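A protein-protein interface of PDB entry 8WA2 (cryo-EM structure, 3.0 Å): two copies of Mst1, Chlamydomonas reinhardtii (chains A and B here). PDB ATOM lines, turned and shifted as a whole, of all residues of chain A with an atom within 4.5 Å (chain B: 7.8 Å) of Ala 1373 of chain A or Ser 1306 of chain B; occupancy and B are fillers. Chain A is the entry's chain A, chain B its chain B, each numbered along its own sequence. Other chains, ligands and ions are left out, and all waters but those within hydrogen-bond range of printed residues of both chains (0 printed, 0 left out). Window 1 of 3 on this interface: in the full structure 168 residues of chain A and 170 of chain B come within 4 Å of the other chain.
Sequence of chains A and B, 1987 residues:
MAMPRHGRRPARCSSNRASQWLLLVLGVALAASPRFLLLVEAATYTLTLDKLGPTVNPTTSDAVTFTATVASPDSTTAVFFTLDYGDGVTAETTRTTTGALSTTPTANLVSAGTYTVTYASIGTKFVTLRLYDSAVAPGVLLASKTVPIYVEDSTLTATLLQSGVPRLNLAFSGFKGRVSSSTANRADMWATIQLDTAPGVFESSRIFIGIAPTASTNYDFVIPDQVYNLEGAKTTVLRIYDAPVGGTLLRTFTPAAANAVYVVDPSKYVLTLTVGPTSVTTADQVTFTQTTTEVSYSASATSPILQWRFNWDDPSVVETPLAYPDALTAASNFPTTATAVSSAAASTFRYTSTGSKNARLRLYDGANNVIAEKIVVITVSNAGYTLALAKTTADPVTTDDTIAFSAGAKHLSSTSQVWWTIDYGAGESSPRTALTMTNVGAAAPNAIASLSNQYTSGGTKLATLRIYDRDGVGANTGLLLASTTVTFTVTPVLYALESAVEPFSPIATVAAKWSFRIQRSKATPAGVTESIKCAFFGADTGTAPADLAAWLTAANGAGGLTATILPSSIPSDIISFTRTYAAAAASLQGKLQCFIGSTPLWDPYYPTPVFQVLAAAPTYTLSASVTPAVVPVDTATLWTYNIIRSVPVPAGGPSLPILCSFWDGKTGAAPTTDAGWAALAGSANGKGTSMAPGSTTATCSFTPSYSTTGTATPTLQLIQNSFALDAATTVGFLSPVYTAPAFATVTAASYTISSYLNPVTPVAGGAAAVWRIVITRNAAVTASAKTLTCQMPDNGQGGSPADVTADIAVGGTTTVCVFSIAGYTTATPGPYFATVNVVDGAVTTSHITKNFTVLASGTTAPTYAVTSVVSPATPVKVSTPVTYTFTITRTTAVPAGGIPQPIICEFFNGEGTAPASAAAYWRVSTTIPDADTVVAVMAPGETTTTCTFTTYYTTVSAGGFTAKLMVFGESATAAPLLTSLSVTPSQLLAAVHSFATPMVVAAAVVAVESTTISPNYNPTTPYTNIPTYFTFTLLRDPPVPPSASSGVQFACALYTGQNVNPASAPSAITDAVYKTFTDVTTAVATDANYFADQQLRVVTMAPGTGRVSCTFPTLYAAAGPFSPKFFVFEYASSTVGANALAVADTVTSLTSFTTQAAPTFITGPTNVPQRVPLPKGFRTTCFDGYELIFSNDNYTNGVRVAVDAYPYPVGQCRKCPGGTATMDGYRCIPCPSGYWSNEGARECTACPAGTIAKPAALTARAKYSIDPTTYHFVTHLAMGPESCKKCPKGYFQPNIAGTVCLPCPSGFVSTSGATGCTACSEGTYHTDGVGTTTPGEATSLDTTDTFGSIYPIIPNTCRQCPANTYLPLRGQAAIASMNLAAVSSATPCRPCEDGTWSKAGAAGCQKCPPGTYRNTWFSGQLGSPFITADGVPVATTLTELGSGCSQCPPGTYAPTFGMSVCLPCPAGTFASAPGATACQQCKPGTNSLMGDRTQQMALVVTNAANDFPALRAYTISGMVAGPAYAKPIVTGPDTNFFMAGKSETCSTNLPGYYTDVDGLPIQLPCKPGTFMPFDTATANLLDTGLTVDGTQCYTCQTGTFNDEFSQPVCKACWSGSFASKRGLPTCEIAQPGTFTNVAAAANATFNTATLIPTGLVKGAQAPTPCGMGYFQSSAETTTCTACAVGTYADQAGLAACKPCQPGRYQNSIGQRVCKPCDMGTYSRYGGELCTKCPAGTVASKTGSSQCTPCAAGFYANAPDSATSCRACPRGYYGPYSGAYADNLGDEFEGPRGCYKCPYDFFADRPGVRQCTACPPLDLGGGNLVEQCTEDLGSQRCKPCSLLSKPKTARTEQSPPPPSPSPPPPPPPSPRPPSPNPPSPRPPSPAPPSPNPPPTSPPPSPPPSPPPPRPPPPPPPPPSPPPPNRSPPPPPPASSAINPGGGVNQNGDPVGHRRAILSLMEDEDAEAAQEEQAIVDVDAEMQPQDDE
The backbone carbonyl oxygen (O) of Ala 1374 of chain A sits close to the backbone carbonyl oxygen (O) of Ala 1374 of chain B.
O of Ala 1374 of chain A lies within hydrogen-bond range of N of Ala 1376 of chain B (2.6 Å).
The backbone carbonyl oxygen (O) of Ala 1373 of chain A is in hydrogen-bond range of the side-chain hydroxyl (OG) of Ser 1306 of chain B.
The backbone NH of Ser 1306 of chain A lies within hydrogen-bond range of the side-chain amide oxygen of Gln 1372 of chain B, at 3.2 Å.
OG of Ser 1306 of chain A lies within hydrogen-bond range of O of Ala 1373 of chain B, at 2.9 Å.
OE1 of Gln 1372 of chain A lies within hydrogen-bond range of N of Ser 1306 of chain B (3.2 Å).
The backbone carbonyl oxygen of Gln 1372 of chain A lies within hydrogen-bond range of the backbone NH of His 1326 of chain A, at 2.6 Å.
N of His 1326 of chain B sits at hydrogen-bond distance from O of Gln 1372 of chain B.
N of Ala 1374 of chain A is in hydrogen-bond range of O of His 1326 of chain A, 3.1 Å away.
A ring nitrogen (ND1) of His 1326 of chain A sits at hydrogen-bond distance from the backbone NH (N) of Gly 1307 of chain A, 3.3 Å away.
N of Gly 1307 of chain B lies within hydrogen-bond range of ND1 of His 1326 of chain B (3.2 Å).
N of Ala 1374 of chain B is in hydrogen-bond range of O of His 1326 of chain B (3.1 Å).
Among the printed residues, pairs that only touch across the chains: His 1326 of chain A with Ile 1375 of chain B (3.3 Å), Ser 1306 of chain A with Ile 1375 of chain B (3.3 Å), Ile 1375 of chain A with Ser 1306 of chain B (3.5 Å), Ala 1374 of chain A with Ile 1375 of chain B (3.5 Å), Ile 1375 of chain A with Ala 1374 of chain B (3.5 Å), Ile 1375 of chain A with His 1326 of chain B (3.6 Å), Ile 1375 of chain A with Ala 1376 of chain B (3.6 Å), Gln 1372 of chain A with Pro 1305 of chain B (3.7 Å), Ile 1375 of chain A with Ala 1373 of chain B (3.8 Å) and Ala 1373 of chain A with Ile 1375 of chain B (3.9 Å).
Of the printed residues of chain B, Ala 1373 of chain A touches Ser 1306 and Ile 1375.
Ser 1306 of chain B touches just these residues of chain A: Gln 1372 (3.2 Å), Ala 1373 (2.5 Å) and Ile 1375 (3.5 Å).
Printed residues of chain B within 4 Å of Ala 1374 of chain A: Ala 1374, Ile 1375 and Ala 1376.
Of the printed residues of chain A, Ala 1376 of chain B touches Ala 1374 and Ile 1375.
Printed residues of chain A within 4 Å of Gln 1372 of chain B: Ser 1306.
Of the printed residues of chain B, Ser 1306 of chain A touches Gln 1372, Ala 1373 and Ile 1375.
Cys 1304 of chain B touches none of the printed residues of chain A.
The nearest residue of chain B that does not touch Ala 1373 of chain A is Ala 1373 of chain B (5.1 Å).
Hydrophobic or aromatic side chains of chain B within 4 Å of the printed part of chain A: Pro 1305, His 1326, Ala 1373, Ile 1375 and Ala 1376.
Of the 9 printed residues of chain A, 6 touch a printed residue of chain B.
Ser 1306 of chain A touches Gln 1372 of chain B, and with the chains exchanged Gln 1372 of chain A touches Ser 1306 of chain B.
His 1326 of chain A touches Ile 1375 of chain B, and with the chains exchanged Ile 1375 of chain A touches His 1326 of chain B.
Ala 1373 of chain A touches Ile 1375 of chain B, and with the chains exchanged Ile 1375 of chain A touches Ala 1373 of chain B.
Ala 1374 of chain A touches its own counterpart, Ala 1374 of chain B.
8 positions are printed for both chains.
Of the 16 pairs that touch across the chains among the printed residues, 13 have their exchanged pair printed and touching as well.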
ATOM      1  N   SER A1306     -23.565  16.088 -20.874  1.00  0.00           N
ATOM      2  CA  SER A1306     -23.478  14.689 -21.268  1.00  0.00           C
ATOM      3  C   SER A1306     -23.324  13.792 -20.047  1.00  0.00           C
ATOM      4  O   SER A1306     -22.488  14.045 -19.176  1.00  0.00           O
ATOM      5  CB  SER A1306     -22.304  14.488 -22.222  1.00  0.00           C
ATOM      6  OG  SER A1306     -22.533  13.386 -23.077  1.00  0.00           O
ATOM      7  N   GLY A1307     -24.133  12.739 -19.991  1.00  0.00           N
ATOM      8  CA  GLY A1307     -24.132  11.845 -18.853  1.00  0.00           C
ATOM      9  C   GLY A1307     -25.065  12.228 -17.728  1.00  0.00           C
ATOM     10  O   GLY A1307     -24.941  11.676 -16.631  1.00  0.00           O
ATOM     11  N   HIS A1326     -25.658   7.172 -20.126  1.00  0.00           N
ATOM     12  CA  HIS A1326     -26.722   8.053 -20.592  1.00  0.00           C
ATOM     13  C   HIS A1326     -27.045   7.760 -22.053  1.00  0.00           C
ATOM     14  O   HIS A1326     -26.190   7.931 -22.928  1.00  0.00           O
ATOM     15  CB  HIS A1326     -26.294   9.506 -20.403  1.00  0.00           C
ATOM     16  CG  HIS A1326     -27.264  10.510 -20.936  1.00  0.00           C
ATOM     17  ND1 HIS A1326     -26.859  11.669 -21.563  1.00  0.00           N
ATOM     18  CD2 HIS A1326     -28.617  10.543 -20.925  1.00  0.00           C
ATOM     19  CE1 HIS A1326     -27.919  12.368 -21.921  1.00  0.00           C
ATOM     20  NE2 HIS A1326     -28.998  11.707 -21.547  1.00  0.00           N
ATOM     21  N   GLY A1371     -21.818   9.496 -14.469  1.00  0.00           N
ATOM     22  CA  GLY A1371     -22.099  10.448 -15.525  1.00  0.00           C
ATOM     23  C   GLY A1371     -21.341  10.166 -16.802  1.00  0.00           C
ATOM     24  O   GLY A1371     -20.470  10.943 -17.206  1.00  0.00           O
ATOM     25  N   GLN A1372     -21.664   9.050 -17.445  1.00  0.00           N
ATOM     26  CA  GLN A1372     -21.068   8.663 -18.711  1.00  0.00           C
ATOM     27  C   GLN A1372     -22.168   8.499 -19.747  1.00  0.00           C
ATOM     28  O   GLN A1372     -23.298   8.131 -19.420  1.00  0.00           O
ATOM     29  CB  GLN A1372     -20.278   7.363 -18.582  1.00  0.00           C
ATOM     30  CG  GLN A1372     -19.201   7.405 -17.521  1.00  0.00           C
ATOM     31  CD  GLN A1372     -17.878   7.888 -18.060  1.00  0.00           C
ATOM     32  OE1 GLN A1372     -17.365   7.356 -19.041  1.00  0.00           O
ATOM     33  NE2 GLN A1372     -17.308   8.896 -17.412  1.00  0.00           N
ATOM     34  N   ALA A1373     -21.833   8.778 -21.001  1.00  0.00           N
ATOM     35  CA  ALA A1373     -22.815   8.801 -22.070  1.00  0.00           C
ATOM     36  C   ALA A1373     -22.340   7.956 -23.240  1.00  0.00           C
ATOM     37  O   ALA A1373     -21.139   7.814 -23.478  1.00  0.00           O
ATOM     38  CB  ALA A1373     -23.086  10.230 -22.546  1.00  0.00           C
ATOM     39  N   ALA A1374     -23.300   7.393 -23.966  1.00  0.00           N
ATOM     40  CA  ALA A1374     -22.990   6.689 -25.201  1.00  0.00           C
ATOM     41  C   ALA A1374     -22.614   7.701 -26.273  1.00  0.00           C
ATOM     42  O   ALA A1374     -23.421   8.566 -26.628  1.00  0.00           O
ATOM     43  CB  ALA A1374     -24.181   5.847 -25.645  1.00  0.00           C
ATOM     44  N   ILE A1375     -21.386   7.605 -26.778  1.00  0.00           N
ATOM     45  CA  ILE A1375     -20.898   8.572 -27.753  1.00  0.00           C
ATOM     46  C   ILE A1375     -21.562   8.313 -29.096  1.00  0.00           C
ATOM     47  O   ILE A1375     -21.653   7.166 -29.552  1.00  0.00           O
ATOM     48  CB  ILE A1375     -19.368   8.509 -27.860  1.00  0.00           C
ATOM     49  CG1 ILE A1375     -18.721   8.888 -26.528  1.00  0.00           C
ATOM     50  CG2 ILE A1375     -18.875   9.430 -28.955  1.00  0.00           C
ATOM     51  CD1 ILE A1375     -18.439   7.713 -25.623  1.00  0.00           C
ATOM     52  N   PRO A1388     -19.492   3.527 -23.548  1.00  0.00           N
ATOM     53  CA  PRO A1388     -18.214   3.512 -22.827  1.00  0.00           C
ATOM     54  C   PRO A1388     -18.146   2.466 -21.716  1.00  0.00           C
ATOM     55  O   PRO A1388     -17.669   2.735 -20.614  1.00  0.00           O
ATOM     56  CB  PRO A1388     -18.136   4.932 -22.262  1.00  0.00           C
ATOM     57  CG  PRO A1388     -19.562   5.277 -21.988  1.00  0.00           C
ATOM     58  CD  PRO A1388     -20.418   4.528 -22.989  1.00  0.00           C
ATOM     59  N   PRO B1303     -12.275   1.120 -23.656  1.00  0.00           N
ATOM     60  CA  PRO B1303     -12.695   2.279 -24.452  1.00  0.00           C
ATOM     61  C   PRO B1303     -12.524   3.565 -23.659  1.00  0.00           C
ATOM     62  O   PRO B1303     -12.633   3.583 -22.432  1.00  0.00           O
ATOM     63  CB  PRO B1303     -14.172   2.005 -24.757  1.00  0.00           C
ATOM     64  CG  PRO B1303     -14.561   0.821 -23.965  1.00  0.00           C
ATOM     65  CD  PRO B1303     -13.343   0.124 -23.476  1.00  0.00           C
ATOM     66  N   CYS B1304     -12.239   4.647 -24.379  1.00  0.00           N
ATOM     67  CA  CYS B1304     -12.029   5.928 -23.727  1.00  0.00           C
ATOM     68  C   CYS B1304     -13.298   6.363 -22.999  1.00  0.00           C
ATOM     69  O   CYS B1304     -14.411   6.087 -23.454  1.00  0.00           O
ATOM     70  CB  CYS B1304     -11.625   6.993 -24.743  1.00  0.00           C
ATOM     71  SG  CYS B1304      -9.885   6.967 -25.209  1.00  0.00           S
ATOM     72  N   PRO B1305     -13.159   7.032 -21.857  1.00  0.00           N
ATOM     73  CA  PRO B1305     -14.339   7.543 -21.159  1.00  0.00           C
ATOM     74  C   PRO B1305     -15.077   8.556 -22.019  1.00  0.00           C
ATOM     75  O   PRO B1305     -14.512   9.171 -22.925  1.00  0.00           O
ATOM     76  CB  PRO B1305     -13.759   8.199 -19.901  1.00  0.00           C
ATOM     77  CG  PRO B1305     -12.418   7.589 -19.731  1.00  0.00           C
ATOM     78  CD  PRO B1305     -11.919   7.285 -21.107  1.00  0.00           C
ATOM     79  N   SER B1306     -16.365   8.717 -21.728  1.00  0.00           N
ATOM     80  CA  SER B1306     -17.222   9.573 -22.535  1.00  0.00           C
ATOM     81  C   SER B1306     -16.707  11.005 -22.543  1.00  0.00           C
ATOM     82  O   SER B1306     -16.760  11.698 -21.522  1.00  0.00           O
ATOM     83  CB  SER B1306     -18.655   9.529 -22.011  1.00  0.00           C
ATOM     84  OG  SER B1306     -19.584   9.732 -23.058  1.00  0.00           O
ATOM     85  N   GLY B1307     -16.210  11.452 -23.690  1.00  0.00           N
ATOM     86  CA  GLY B1307     -15.670  12.785 -23.827  1.00  0.00           C
ATOM     87  C   GLY B1307     -14.163  12.878 -23.886  1.00  0.00           C
ATOM     88  O   GLY B1307     -13.630  13.986 -23.776  1.00  0.00           O
ATOM     89  N   PHE B1308     -13.462  11.760 -24.058  1.00  0.00           N
ATOM     90  CA  PHE B1308     -12.008  11.741 -24.082  1.00  0.00           C
ATOM     91  C   PHE B1308     -11.522  11.073 -25.361  1.00  0.00           C
ATOM     92  O   PHE B1308     -12.226  10.265 -25.972  1.00  0.00           O
ATOM     93  CB  PHE B1308     -11.433  11.015 -22.860  1.00  0.00           C
ATOM     94  CG  PHE B1308     -11.621  11.756 -21.569  1.00  0.00           C
ATOM     95  CD1 PHE B1308     -12.872  11.865 -20.991  1.00  0.00           C
ATOM     96  CD2 PHE B1308     -10.545  12.345 -20.933  1.00  0.00           C
ATOM     97  CE1 PHE B1308     -13.044  12.545 -19.809  1.00  0.00           C
ATOM     98  CE2 PHE B1308     -10.711  13.025 -19.750  1.00  0.00           C
ATOM     99  CZ  PHE B1308     -11.961  13.126 -19.187  1.00  0.00           C
ATOM    100  N   VAL B1309     -10.298  11.421 -25.762  1.00  0.00           N
ATOM    101  CA  VAL B1309      -9.697  10.928 -26.994  1.00  0.00           C
ATOM    102  C   VAL B1309      -8.307  10.391 -26.680  1.00  0.00           C
ATOM    103  O   VAL B1309      -7.724  10.687 -25.635  1.00  0.00           O
ATOM    104  CB  VAL B1309      -9.614  12.019 -28.081  1.00  0.00           C
ATOM    105  CG1 VAL B1309     -10.986  12.614 -28.341  1.00  0.00           C
ATOM    106  CG2 VAL B1309      -8.630  13.095 -27.673  1.00  0.00           C
ATOM    107  N   ALA B1319      -9.052  15.041 -22.687  1.00  0.00           N
ATOM    108  CA  ALA B1319     -10.423  15.521 -22.773  1.00  0.00           C
ATOM    109  C   ALA B1319     -10.572  16.552 -23.882  1.00  0.00           C
ATOM    110  O   ALA B1319      -9.678  17.370 -24.114  1.00  0.00           O
ATOM    111  CB  ALA B1319     -10.860  16.129 -21.440  1.00  0.00           C
ATOM    112  N   CYS B1320     -11.712  16.501 -24.570  1.00  0.00           N
ATOM    113  CA  CYS B1320     -12.026  17.510 -25.571  1.00  0.00           C
ATOM    114  C   CYS B1320     -12.126  18.878 -24.905  1.00  0.00           C
ATOM    115  O   CYS B1320     -12.751  19.023 -23.850  1.00  0.00           O
ATOM    116  CB  CYS B1320     -13.338  17.167 -26.279  1.00  0.00           C
ATOM    117  SG  CYS B1320     -13.266  15.825 -27.505  1.00  0.00           S
ATOM    118  N   HIS B1326     -17.108  15.555 -28.101  1.00  0.00           N
ATOM    119  CA  HIS B1326     -16.529  14.301 -28.566  1.00  0.00           C
ATOM    120  C   HIS B1326     -17.524  13.564 -29.457  1.00  0.00           C
ATOM    121  O   HIS B1326     -18.633  13.238 -29.024  1.00  0.00           O
ATOM    122  CB  HIS B1326     -16.126  13.447 -27.367  1.00  0.00           C
ATOM    123  CG  HIS B1326     -15.713  12.052 -27.716  1.00  0.00           C
ATOM    124  ND1 HIS B1326     -15.868  10.994 -26.846  1.00  0.00           N
ATOM    125  CD2 HIS B1326     -15.140  11.541 -28.830  1.00  0.00           C
ATOM    126  CE1 HIS B1326     -15.417   9.891 -27.414  1.00  0.00           C
ATOM    127  NE2 HIS B1326     -14.971  10.195 -28.619  1.00  0.00           N
ATOM    128  N   ARG B1370     -15.288  20.938 -20.324  1.00  0.00           N
ATOM    129  CA  ARG B1370     -14.389  20.037 -21.026  1.00  0.00           C
ATOM    130  C   ARG B1370     -14.913  18.610 -20.967  1.00  0.00           C
ATOM    131  O   ARG B1370     -15.549  18.199 -19.994  1.00  0.00           O
ATOM    132  CB  ARG B1370     -12.984  20.090 -20.427  1.00  0.00           C
ATOM    133  CG  ARG B1370     -12.289  21.425 -20.578  1.00  0.00           C
ATOM    134  CD  ARG B1370     -11.020  21.473 -19.748  1.00  0.00           C
ATOM    135  NE  ARG B1370      -9.958  20.655 -20.317  1.00  0.00           N
ATOM    136  CZ  ARG B1370      -9.187  21.023 -21.331  1.00  0.00           C
ATOM    137  NH1 ARG B1370      -9.325  22.203 -21.910  1.00  0.00           N
ATOM    138  NH2 ARG B1370      -8.253  20.186 -21.772  1.00  0.00           N
ATOM    139  N   GLY B1371     -14.635  17.855 -22.024  1.00  0.00           N
ATOM    140  CA  GLY B1371     -15.004  16.456 -22.060  1.00  0.00           C
ATOM    141  C   GLY B1371     -16.496  16.225 -22.151  1.00  0.00           C
ATOM    142  O   GLY B1371     -17.106  15.694 -21.219  1.00  0.00           O
ATOM    143  N   GLN B1372     -17.095  16.621 -23.269  1.00  0.00           N
ATOM    144  CA  GLN B1372     -18.507  16.398 -23.527  1.00  0.00           C
ATOM    145  C   GLN B1372     -18.660  15.623 -24.826  1.00  0.00           C
ATOM    146  O   GLN B1372     -17.858  15.769 -25.751  1.00  0.00           O
ATOM    147  CB  GLN B1372     -19.274  17.718 -23.612  1.00  0.00           C
ATOM    148  CG  GLN B1372     -19.063  18.628 -22.422  1.00  0.00           C
ATOM    149  CD  GLN B1372     -20.002  18.316 -21.282  1.00  0.00           C
ATOM    150  OE1 GLN B1372     -21.189  18.076 -21.490  1.00  0.00           O
ATOM    151  NE2 GLN B1372     -19.474  18.322 -20.065  1.00  0.00           N
ATOM    152  N   ALA B1373     -19.696  14.797 -24.891  1.00  0.00           N
ATOM    153  CA  ALA B1373     -19.889  13.895 -26.014  1.00  0.00           C
ATOM    154  C   ALA B1373     -21.309  14.010 -26.542  1.00  0.00           C
ATOM    155  O   ALA B1373     -22.249  14.280 -25.792  1.00  0.00           O
ATOM    156  CB  ALA B1373     -19.605  12.444 -25.618  1.00  0.00           C
ATOM    157  N   ALA B1374     -21.454  13.802 -27.847  1.00  0.00           N
ATOM    158  CA  ALA B1374     -22.777  13.710 -28.445  1.00  0.00           C
ATOM    159  C   ALA B1374     -23.469  12.455 -27.932  1.00  0.00           C
ATOM    160  O   ALA B1374     -22.992  11.340 -28.161  1.00  0.00           O
ATOM    161  CB  ALA B1374     -22.674  13.688 -29.967  1.00  0.00           C
ATOM    162  N   ILE B1375     -24.582  12.636 -27.225  1.00  0.00           N
ATOM    163  CA  ILE B1375     -25.264  11.505 -26.607  1.00  0.00           C
ATOM    164  C   ILE B1375     -25.949  10.683 -27.686  1.00  0.00           C
ATOM    165  O   ILE B1375     -26.696  11.216 -28.516  1.00  0.00           O
ATOM    166  CB  ILE B1375     -26.265  11.988 -25.550  1.00  0.00           C
ATOM    167  CG1 ILE B1375     -25.535  12.686 -24.400  1.00  0.00           C
ATOM    168  CG2 ILE B1375     -27.079  10.820 -25.028  1.00  0.00           C
ATOM    169  CD1 ILE B1375     -25.373  14.176 -24.586  1.00  0.00           C
ATOM    170  N   ALA B1376     -25.699   9.380 -27.679  1.00  0.00           N
ATOM    171  CA  ALA B1376     -26.131   8.534 -28.777  1.00  0.00           C
ATOM    172  C   ALA B1376     -27.559   8.048 -28.574  1.00  0.00           C
ATOM    173  O   ALA B1376     -28.107   8.064 -27.470  1.00  0.00           O
ATOM    174  CB  ALA B1376     -25.195   7.337 -28.935  1.00  0.00           C
